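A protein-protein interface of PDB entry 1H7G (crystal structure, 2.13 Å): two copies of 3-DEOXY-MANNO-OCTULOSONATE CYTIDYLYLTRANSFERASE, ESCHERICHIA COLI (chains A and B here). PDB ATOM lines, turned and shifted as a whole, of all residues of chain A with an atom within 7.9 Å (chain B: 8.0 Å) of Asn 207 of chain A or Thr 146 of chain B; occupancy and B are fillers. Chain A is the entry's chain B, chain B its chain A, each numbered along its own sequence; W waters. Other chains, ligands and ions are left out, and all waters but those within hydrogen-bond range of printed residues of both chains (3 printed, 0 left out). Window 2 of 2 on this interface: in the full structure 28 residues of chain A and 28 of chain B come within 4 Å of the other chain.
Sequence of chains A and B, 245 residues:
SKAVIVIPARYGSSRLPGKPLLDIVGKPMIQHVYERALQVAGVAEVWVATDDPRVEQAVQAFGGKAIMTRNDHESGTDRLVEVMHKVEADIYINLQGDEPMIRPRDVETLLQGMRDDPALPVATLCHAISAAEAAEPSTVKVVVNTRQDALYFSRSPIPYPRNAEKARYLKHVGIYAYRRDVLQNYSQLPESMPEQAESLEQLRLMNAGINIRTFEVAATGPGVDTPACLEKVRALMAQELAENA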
ATOM      1  N   LEU A 189      28.123 -12.829 -17.045  1.00  0.00           N
ATOM      2  CA  LEU A 189      27.926 -13.047 -18.481  1.00  0.00           C
ATOM      3  C   LEU A 189      28.899 -14.069 -19.052  1.00  0.00           C
ATOM      4  O   LEU A 189      30.116 -13.955 -18.855  1.00  0.00           O
ATOM      5  CB  LEU A 189      28.070 -11.734 -19.255  1.00  0.00           C
ATOM      6  CG  LEU A 189      27.216 -10.532 -18.841  1.00  0.00           C
ATOM      7  CD1 LEU A 189      27.418  -9.430 -19.850  1.00  0.00           C
ATOM      8  CD2 LEU A 189      25.748 -10.905 -18.763  1.00  0.00           C
ATOM      9  N   PRO A 190      28.379 -15.078 -19.786  1.00  0.00           N
ATOM     10  CA  PRO A 190      29.219 -16.121 -20.390  1.00  0.00           C
ATOM     11  C   PRO A 190      29.890 -15.643 -21.683  1.00  0.00           C
ATOM     12  O   PRO A 190      29.337 -14.805 -22.397  1.00  0.00           O
ATOM     13  CB  PRO A 190      28.211 -17.226 -20.680  1.00  0.00           C
ATOM     14  CG  PRO A 190      26.990 -16.454 -21.067  1.00  0.00           C
ATOM     15  CD  PRO A 190      26.947 -15.351 -20.027  1.00  0.00           C
ATOM     16  N   GLU A 191      31.092 -16.143 -21.967  1.00  0.00           N
ATOM     17  CA  GLU A 191      31.790 -15.773 -23.200  1.00  0.00           C
ATOM     18  C   GLU A 191      30.956 -16.306 -24.349  1.00  0.00           C
ATOM     19  O   GLU A 191      30.324 -17.352 -24.222  1.00  0.00           O
ATOM     20  CB  GLU A 191      33.183 -16.394 -23.269  1.00  0.00           C
ATOM     21  CG  GLU A 191      34.200 -15.817 -22.291  1.00  0.00           C
ATOM     22  CD  GLU A 191      35.604 -16.355 -22.535  1.00  0.00           C
ATOM     23  OE1 GLU A 191      35.960 -16.556 -23.715  1.00  0.00           O
ATOM     24  OE2 GLU A 191      36.346 -16.584 -21.555  1.00  0.00           O
ATOM     25  N   SER A 192      30.938 -15.587 -25.462  1.00  0.00           N
ATOM     26  CA  SER A 192      30.137 -16.014 -26.596  1.00  0.00           C
ATOM     27  C   SER A 192      30.964 -16.553 -27.745  1.00  0.00           C
ATOM     28  O   SER A 192      32.159 -16.275 -27.853  1.00  0.00           O
ATOM     29  CB  SER A 192      29.258 -14.860 -27.093  1.00  0.00           C
ATOM     30  OG  SER A 192      30.032 -13.794 -27.621  1.00  0.00           O
ATOM     31  N   MET A 193      30.322 -17.340 -28.601  1.00  0.00           N
ATOM     32  CA  MET A 193      31.003 -17.895 -29.760  1.00  0.00           C
ATOM     33  C   MET A 193      31.514 -16.767 -30.675  1.00  0.00           C
ATOM     34  O   MET A 193      32.680 -16.795 -31.090  1.00  0.00           O
ATOM     35  CB  MET A 193      30.084 -18.873 -30.504  1.00  0.00           C
ATOM     36  CG  MET A 193      30.709 -19.533 -31.732  1.00  0.00           C
ATOM     37  SD  MET A 193      30.716 -18.439 -33.163  1.00  0.00           S
ATOM     38  CE  MET A 193      28.971 -18.520 -33.677  1.00  0.00           C
ATOM     39  N   PRO A 194      30.662 -15.760 -30.996  1.00  0.00           N
ATOM     40  CA  PRO A 194      31.131 -14.666 -31.863  1.00  0.00           C
ATOM     41  C   PRO A 194      32.281 -13.885 -31.214  1.00  0.00           C
ATOM     42  O   PRO A 194      33.212 -13.466 -31.899  1.00  0.00           O
ATOM     43  CB  PRO A 194      29.874 -13.797 -32.036  1.00  0.00           C
ATOM     44  CG  PRO A 194      28.767 -14.804 -31.982  1.00  0.00           C
ATOM     45  CD  PRO A 194      29.197 -15.671 -30.812  1.00  0.00           C
ATOM     46  N   GLU A 195      32.222 -13.703 -29.897  1.00  0.00           N
ATOM     47  CA  GLU A 195      33.285 -12.996 -29.192  1.00  0.00           C
ATOM     48  C   GLU A 195      34.628 -13.725 -29.327  1.00  0.00           C
ATOM     49  O   GLU A 195      35.652 -13.112 -29.625  1.00  0.00           O
ATOM     50  CB  GLU A 195      32.957 -12.865 -27.711  1.00  0.00           C
ATOM     51  CG  GLU A 195      34.104 -12.268 -26.907  1.00  0.00           C
ATOM     52  CD  GLU A 195      33.962 -12.490 -25.424  1.00  0.00           C
ATOM     53  OE1 GLU A 195      32.890 -12.959 -24.987  1.00  0.00           O
ATOM     54  OE2 GLU A 195      34.930 -12.199 -24.694  1.00  0.00           O
ATOM     55  N   GLU A 201      35.601  -8.416 -27.207  1.00  0.00           N
ATOM     56  CA  GLU A 201      34.926  -8.513 -25.920  1.00  0.00           C
ATOM     57  C   GLU A 201      33.560  -7.843 -25.843  1.00  0.00           C
ATOM     58  O   GLU A 201      32.698  -8.306 -25.104  1.00  0.00           O
ATOM     59  CB  GLU A 201      35.842  -7.976 -24.815  1.00  0.00           C
ATOM     60  CG  GLU A 201      35.306  -8.162 -23.406  1.00  0.00           C
ATOM     61  CD  GLU A 201      36.263  -7.655 -22.330  1.00  0.00           C
ATOM     62  OE1 GLU A 201      37.040  -6.710 -22.598  1.00  0.00           O
ATOM     63  OE2 GLU A 201      36.227  -8.201 -21.209  1.00  0.00           O
ATOM     64  N   GLN A 202      33.356  -6.753 -26.579  1.00  0.00           N
ATOM     65  CA  GLN A 202      32.060  -6.074 -26.556  1.00  0.00           C
ATOM     66  C   GLN A 202      30.914  -6.978 -27.030  1.00  0.00           C
ATOM     67  O   GLN A 202      29.753  -6.725 -26.712  1.00  0.00           O
ATOM     68  CB  GLN A 202      32.084  -4.782 -27.373  1.00  0.00           C
ATOM     69  CG  GLN A 202      32.363  -4.957 -28.855  1.00  0.00           C
ATOM     70  CD  GLN A 202      33.839  -4.864 -29.187  1.00  0.00           C
ATOM     71  OE1 GLN A 202      34.675  -5.486 -28.533  1.00  0.00           O
ATOM     72  NE2 GLN A 202      34.167  -4.072 -30.202  1.00  0.00           N
ATOM     73  N   LEU A 203      31.251  -8.045 -27.757  1.00  0.00           N
ATOM     74  CA  LEU A 203      30.250  -8.999 -28.252  1.00  0.00           C
ATOM     75  C   LEU A 203      29.658  -9.857 -27.128  1.00  0.00           C
ATOM     76  O   LEU A 203      28.635 -10.508 -27.316  1.00  0.00           O
ATOM     77  CB  LEU A 203      30.833  -9.896 -29.358  1.00  0.00           C
ATOM     78  CG  LEU A 203      31.243  -9.177 -30.648  1.00  0.00           C
ATOM     79  CD1 LEU A 203      31.874 -10.138 -31.633  1.00  0.00           C
ATOM     80  CD2 LEU A 203      30.036  -8.502 -31.264  1.00  0.00           C
ATOM     81  N   ARG A 204      30.297  -9.859 -25.960  1.00  0.00           N
ATOM     82  CA  ARG A 204      29.777 -10.621 -24.825  1.00  0.00           C
ATOM     83  C   ARG A 204      28.495  -9.929 -24.384  1.00  0.00           C
ATOM     84  O   ARG A 204      27.544 -10.575 -23.939  1.00  0.00           O
ATOM     85  CB  ARG A 204      30.776 -10.636 -23.658  1.00  0.00           C
ATOM     86  CG  ARG A 204      30.446 -11.670 -22.582  1.00  0.00           C
ATOM     87  CD  ARG A 204      31.497 -11.730 -21.488  1.00  0.00           C
ATOM     88  NE  ARG A 204      32.845 -11.924 -22.018  1.00  0.00           N
ATOM     89  CZ  ARG A 204      33.956 -11.862 -21.288  1.00  0.00           C
ATOM     90  NH1 ARG A 204      33.891 -11.626 -19.989  1.00  0.00           N
ATOM     91  NH2 ARG A 204      35.142 -11.947 -21.874  1.00  0.00           N
ATOM     92  N   LEU A 205      28.489  -8.608 -24.523  1.00  0.00           N
ATOM     93  CA  LEU A 205      27.343  -7.773 -24.157  1.00  0.00           C
ATOM     94  C   LEU A 205      26.164  -7.989 -25.108  1.00  0.00           C
ATOM     95  O   LEU A 205      25.027  -8.180 -24.674  1.00  0.00           O
ATOM     96  CB  LEU A 205      27.759  -6.294 -24.167  1.00  0.00           C
ATOM     97  CG  LEU A 205      28.880  -5.882 -23.204  1.00  0.00           C
ATOM     98  CD1 LEU A 205      29.376  -4.496 -23.554  1.00  0.00           C
ATOM     99  CD2 LEU A 205      28.393  -5.940 -21.750  1.00  0.00           C
ATOM    100  N   MET A 206      26.443  -7.969 -26.406  1.00  0.00           N
ATOM    101  CA  MET A 206      25.408  -8.157 -27.420  1.00  0.00           C
ATOM    102  C   MET A 206      24.784  -9.539 -27.349  1.00  0.00           C
ATOM    103  O   MET A 206      23.599  -9.695 -27.608  1.00  0.00           O
ATOM    104  CB  MET A 206      25.983  -7.934 -28.809  1.00  0.00           C
ATOM    105  CG  MET A 206      26.647  -6.583 -28.974  1.00  0.00           C
ATOM    106  SD  MET A 206      26.701  -6.142 -30.705  1.00  0.00           S
ATOM    107  CE  MET A 206      25.102  -5.473 -30.880  1.00  0.00           C
ATOM    108  N   ASN A 207      25.595 -10.538 -27.012  1.00  0.00           N
ATOM    109  CA  ASN A 207      25.120 -11.908 -26.886  1.00  0.00           C
ATOM    110  C   ASN A 207      24.077 -11.993 -25.771  1.00  0.00           C
ATOM    111  O   ASN A 207      23.120 -12.756 -25.866  1.00  0.00           O
ATOM    112  CB  ASN A 207      26.294 -12.842 -26.588  1.00  0.00           C
ATOM    113  CG  ASN A 207      25.872 -14.289 -26.448  1.00  0.00           C
ATOM    114  OD1 ASN A 207      25.538 -14.948 -27.430  1.00  0.00           O
ATOM    115  ND2 ASN A 207      25.892 -14.795 -25.220  1.00  0.00           N
ATOM    116  N   ALA A 208      24.245 -11.175 -24.737  1.00  0.00           N
ATOM    117  CA  ALA A 208      23.326 -11.151 -23.607  1.00  0.00           C
ATOM    118  C   ALA A 208      22.099 -10.283 -23.859  1.00  0.00           C
ATOM    119  O   ALA A 208      21.222 -10.188 -23.008  1.00  0.00           O
ATOM    120  CB  ALA A 208      24.054 -10.665 -22.364  1.00  0.00           C
ATOM    121  N   GLY A 209      22.058  -9.618 -25.007  1.00  0.00           N
ATOM    122  CA  GLY A 209      20.933  -8.760 -25.323  1.00  0.00           C
ATOM    123  C   GLY A 209      21.025  -7.369 -24.721  1.00  0.00           C
ATOM    124  O   GLY A 209      20.012  -6.687 -24.560  1.00  0.00           O
ATOM    125  N   ILE A 210      22.233  -6.946 -24.368  1.00  0.00           N
ATOM    126  CA  ILE A 210      22.429  -5.619 -23.793  1.00  0.00           C
ATOM    127  C   ILE A 210      22.669  -4.652 -24.947  1.00  0.00           C
ATOM    128  O   ILE A 210      23.566  -4.863 -25.768  1.00  0.00           O
ATOM    129  CB  ILE A 210      23.626  -5.606 -22.802  1.00  0.00           C
ATOM    130  CG1 ILE A 210      23.337  -6.575 -21.643  1.00  0.00           C
ATOM    131  CG2 ILE A 210      23.895  -4.179 -22.291  1.00  0.00           C
ATOM    132  CD1 ILE A 210      24.497  -6.791 -20.712  1.00  0.00           C
ATOM    133  N   ILE A 212      23.863  -1.458 -27.053  1.00  0.00           N
ATOM    134  CA  ILE A 212      25.031  -0.588 -27.111  1.00  0.00           C
ATOM    135  C   ILE A 212      24.755   0.477 -28.172  1.00  0.00           C
ATOM    136  O   ILE A 212      24.668   0.158 -29.357  1.00  0.00           O
ATOM    137  CB  ILE A 212      26.309  -1.385 -27.546  1.00  0.00           C
ATOM    138  CG1 ILE A 212      26.646  -2.480 -26.520  1.00  0.00           C
ATOM    139  CG2 ILE A 212      27.491  -0.433 -27.757  1.00  0.00           C
ATOM    140  CD1 ILE A 212      27.705  -3.452 -26.997  1.00  0.00           C
ATOM    141  N   VAL B 143      24.288 -14.158 -37.461  1.00  0.00           N
ATOM    142  CA  VAL B 143      24.858 -14.321 -36.135  1.00  0.00           C
ATOM    143  C   VAL B 143      23.703 -14.008 -35.175  1.00  0.00           C
ATOM    144  O   VAL B 143      23.009 -13.006 -35.354  1.00  0.00           O
ATOM    145  CB  VAL B 143      26.049 -13.353 -35.902  1.00  0.00           C
ATOM    146  CG1 VAL B 143      26.550 -13.474 -34.461  1.00  0.00           C
ATOM    147  CG2 VAL B 143      27.184 -13.696 -36.864  1.00  0.00           C
ATOM    148  N   VAL B 144      23.483 -14.880 -34.188  1.00  0.00           N
ATOM    149  CA  VAL B 144      22.403 -14.705 -33.218  1.00  0.00           C
ATOM    150  C   VAL B 144      22.917 -14.591 -31.786  1.00  0.00           C
ATOM    151  O   VAL B 144      24.069 -14.918 -31.524  1.00  0.00           O
ATOM    152  CB  VAL B 144      21.401 -15.906 -33.279  1.00  0.00           C
ATOM    153  CG1 VAL B 144      20.866 -16.076 -34.685  1.00  0.00           C
ATOM    154  CG2 VAL B 144      22.065 -17.197 -32.812  1.00  0.00           C
ATOM    155  N   ASN B 145      22.058 -14.121 -30.877  1.00  0.00           N
ATOM    156  CA  ASN B 145      22.381 -13.994 -29.454  1.00  0.00           C
ATOM    157  C   ASN B 145      21.798 -15.196 -28.700  1.00  0.00           C
ATOM    158  O   ASN B 145      21.298 -16.119 -29.334  1.00  0.00           O
ATOM    159  CB  ASN B 145      21.871 -12.647 -28.874  1.00  0.00           C
ATOM    160  CG  ASN B 145      20.342 -12.518 -28.879  1.00  0.00           C
ATOM    161  OD1 ASN B 145      19.613 -13.473 -29.142  1.00  0.00           O
ATOM    162  ND2 ASN B 145      19.858 -11.319 -28.576  1.00  0.00           N
ATOM    163  N   THR B 146      21.851 -15.195 -27.368  1.00  0.00           N
ATOM    164  CA  THR B 146      21.322 -16.320 -26.579  1.00  0.00           C
ATOM    165  C   THR B 146      19.849 -16.640 -26.798  1.00  0.00           C
ATOM    166  O   THR B 146      19.450 -17.798 -26.671  1.00  0.00           O
ATOM    167  CB  THR B 146      21.531 -16.145 -25.052  1.00  0.00           C
ATOM    168  OG1 THR B 146      21.085 -14.846 -24.638  1.00  0.00           O
ATOM    169  CG2 THR B 146      22.975 -16.339 -24.687  1.00  0.00           C
ATOM    170  N   ARG B 147      19.039 -15.621 -27.082  1.00  0.00           N
ATOM    171  CA  ARG B 147      17.606 -15.820 -27.317  1.00  0.00           C
ATOM    172  C   ARG B 147      17.332 -16.216 -28.767  1.00  0.00           C
ATOM    173  O   ARG B 147      16.180 -16.322 -29.190  1.00  0.00           O
ATOM    174  CB  ARG B 147      16.818 -14.551 -26.978  1.00  0.00           C
ATOM    175  CG  ARG B 147      16.725 -14.225 -25.493  1.00  0.00           C
ATOM    176  CD  ARG B 147      15.819 -13.018 -25.262  1.00  0.00           C
ATOM    177  NE  ARG B 147      16.303 -11.818 -25.944  1.00  0.00           N
ATOM    178  CZ  ARG B 147      16.959 -10.824 -25.348  1.00  0.00           C
ATOM    179  NH1 ARG B 147      17.218 -10.876 -24.046  1.00  0.00           N
ATOM    180  NH2 ARG B 147      17.360  -9.776 -26.056  1.00  0.00           N
ATOM    181  N   GLN B 148      18.403 -16.457 -29.511  1.00  0.00           N
ATOM    182  CA  GLN B 148      18.329 -16.831 -30.920  1.00  0.00           C
ATOM    183  C   GLN B 148      17.845 -15.683 -31.802  1.00  0.00           C
ATOM    184  O   GLN B 148      17.377 -15.888 -32.921  1.00  0.00           O
ATOM    185  CB  GLN B 148      17.475 -18.088 -31.113  1.00  0.00           C
ATOM    186  CG  GLN B 148      18.011 -19.290 -30.352  1.00  0.00           C
ATOM    187  CD  GLN B 148      17.287 -20.564 -30.710  1.00  0.00           C
ATOM    188  OE1 GLN B 148      16.053 -20.629 -30.674  1.00  0.00           O
ATOM    189  NE2 GLN B 148      18.049 -21.592 -31.072  1.00  0.00           N
ATOM    190  N   ASP B 149      17.939 -14.472 -31.266  1.00  0.00           N
ATOM    191  CA  ASP B 149      17.559 -13.267 -31.995  1.00  0.00           C
ATOM    192  C   ASP B 149      18.715 -12.923 -32.914  1.00  0.00           C
ATOM    193  O   ASP B 149      19.875 -12.963 -32.491  1.00  0.00           O
ATOM    194  CB  ASP B 149      17.340 -12.100 -31.030  1.00  0.00           C
ATOM    195  CG  ASP B 149      16.036 -12.202 -30.274  1.00  0.00           C
ATOM    196  OD1 ASP B 149      15.164 -13.011 -30.670  1.00  0.00           O
ATOM    197  OD2 ASP B 149      15.882 -11.457 -29.288  1.00  0.00           O
ATOM    198  N   LEU B 151      21.418 -10.860 -34.830  1.00  0.00           N
ATOM    199  CA  LEU B 151      22.195  -9.651 -34.558  1.00  0.00           C
ATOM    200  C   LEU B 151      22.427  -8.932 -35.887  1.00  0.00           C
ATOM    201  O   LEU B 151      22.296  -7.710 -35.982  1.00  0.00           O
ATOM    202  CB  LEU B 151      23.546  -9.998 -33.914  1.00  0.00           C
ATOM    203  CG  LEU B 151      23.533 -10.555 -32.486  1.00  0.00           C
ATOM    204  CD1 LEU B 151      24.956 -10.691 -31.984  1.00  0.00           C
ATOM    205  CD2 LEU B 151      22.757  -9.617 -31.575  1.00  0.00           C
ATOM    206  N   ARG B 213      13.651 -13.417 -34.921  1.00  0.00           N
ATOM    207  CA  ARG B 213      14.193 -14.584 -34.228  1.00  0.00           C
ATOM    208  C   ARG B 213      14.505 -15.674 -35.244  1.00  0.00           C
ATOM    209  O   ARG B 213      13.703 -15.965 -36.131  1.00  0.00           O
ATOM    210  CB  ARG B 213      13.228 -15.097 -33.166  1.00  0.00           C
ATOM    211  CG  ARG B 213      13.783 -16.265 -32.368  1.00  0.00           C
ATOM    212  CD  ARG B 213      13.095 -16.386 -31.023  1.00  0.00           C
ATOM    213  NE  ARG B 213      13.320 -15.192 -30.208  1.00  0.00           N
ATOM    214  CZ  ARG B 213      12.414 -14.643 -29.402  1.00  0.00           C
ATOM    215  NH1 ARG B 213      11.205 -15.185 -29.286  1.00  0.00           N
ATOM    216  NH2 ARG B 213      12.705 -13.524 -28.741  1.00  0.00           N
HETATM  217  O   HOH W   1      20.982  -8.629 -28.637  1.00  0.00           O
HETATM  218  O   HOH W   2      26.064 -13.869 -29.857  1.00  0.00           O
HETATM  219  O   HOH W   3      17.283  -7.417 -23.613  1.00  0.00           O
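N of Thr 146 of chain B is in hydrogen-bond range of O of Asn 207 of chain A, 3.1 Å away.
The guanidinium group of Arg 213 of chain B sits at hydrogen-bond distance from the backbone carbonyl oxygen of Arg 147 of chain B, 3.2 Å away. N of Asp 149 of chain B lies within hydrogen-bond range of OD1 of Asn 145 of chain B, at 2.9 Å. The side-chain amide oxygen (OD1) of Asn 145 of chain B lies within hydrogen-bond range of the backbone NH (N) of Gln 148 of chain B (3.2 Å). The side-chain amide oxygen (OD1) of Asn 145 of chain B sits at hydrogen-bond distance from the backbone NH (N) of Arg 147 of chain B, 3.0 Å away. The backbone carbonyl oxygen of Val 143 of chain B is in hydrogen-bond range of the backbone NH of Leu 151 of chain B (2.7 Å). The guanidinium group (NE) of Arg 147 of chain B is in salt-bridge range of the side-chain carboxylate (OD2) of Asp 149 of chain B.
Pro 194 of chain A touches Val 143 of chain B (CG to CG1, 3.6 Å). O of Met 206 of chain A touches CB of Asn 145 of chain B (3.6 Å). Asn 145 of chain B touches Asn 207 of chain A. CA of Gly 209 of chain A touches NH2 of Arg 147 of chain B (3.8 Å).
Of chain B, only Asn 145 and Thr 146 come within 4 Å of Asn 207 of chain A. Of chain A, only Asn 207 (3.1 Å) comes within 4 Å of Thr 146 of chain B. Of the printed residues of chain B, Pro 194 of chain A touches Val 143. Of the printed residues of chain B, Met 206 of chain A touches Asn 145 (3.6 Å). Of the printed residues of chain A, Val 143 of chain B touches Pro 194. Leu 203 of chain A touches none of the printed residues of chain B. Asp 149 of chain B touches none of the printed residues of chain A. The nearest residue of chain B that does not touch Asn 207 of chain A is Val 144 of chain B (4.3 Å). The nearest residue of chain A that does not touch Thr 146 of chain B is Ala 208 of chain A (4.4 Å). The nearest printed residue of chain B that does not touch Met 206 of chain A is Leu 151 of chain B (4.1 Å).
Of the 18 printed residues of chain A, 4 touch a printed residue of chain B. Of the 9 printed residues of chain B, 4 touch a printed residue of chain A. Among the printed residues, no Asp or Glu carboxylate lies within 4 Å of a Lys or Arg side-chain nitrogen of the other chain.
No position is printed for both chains. Of the 5 pairs that touch across the chains among the printed residues, none has its exchanged pair printed and touching as well.
Water W2 lies within hydrogen-bond range of OD1 of Asn 207 of chain A and O of Val 144 of chain B. Water W1 lies within hydrogen-bond range of ND2 of Asn 145 of chain B (2.9 Å) and O of Met 206 of chain A (3.0 Å). Water W3 bridges the backbone carbonyl oxygen of Gly 209 of chain A (3.0 Å) and the guanidinium group of Arg 147 of chain B (3.4 Å).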
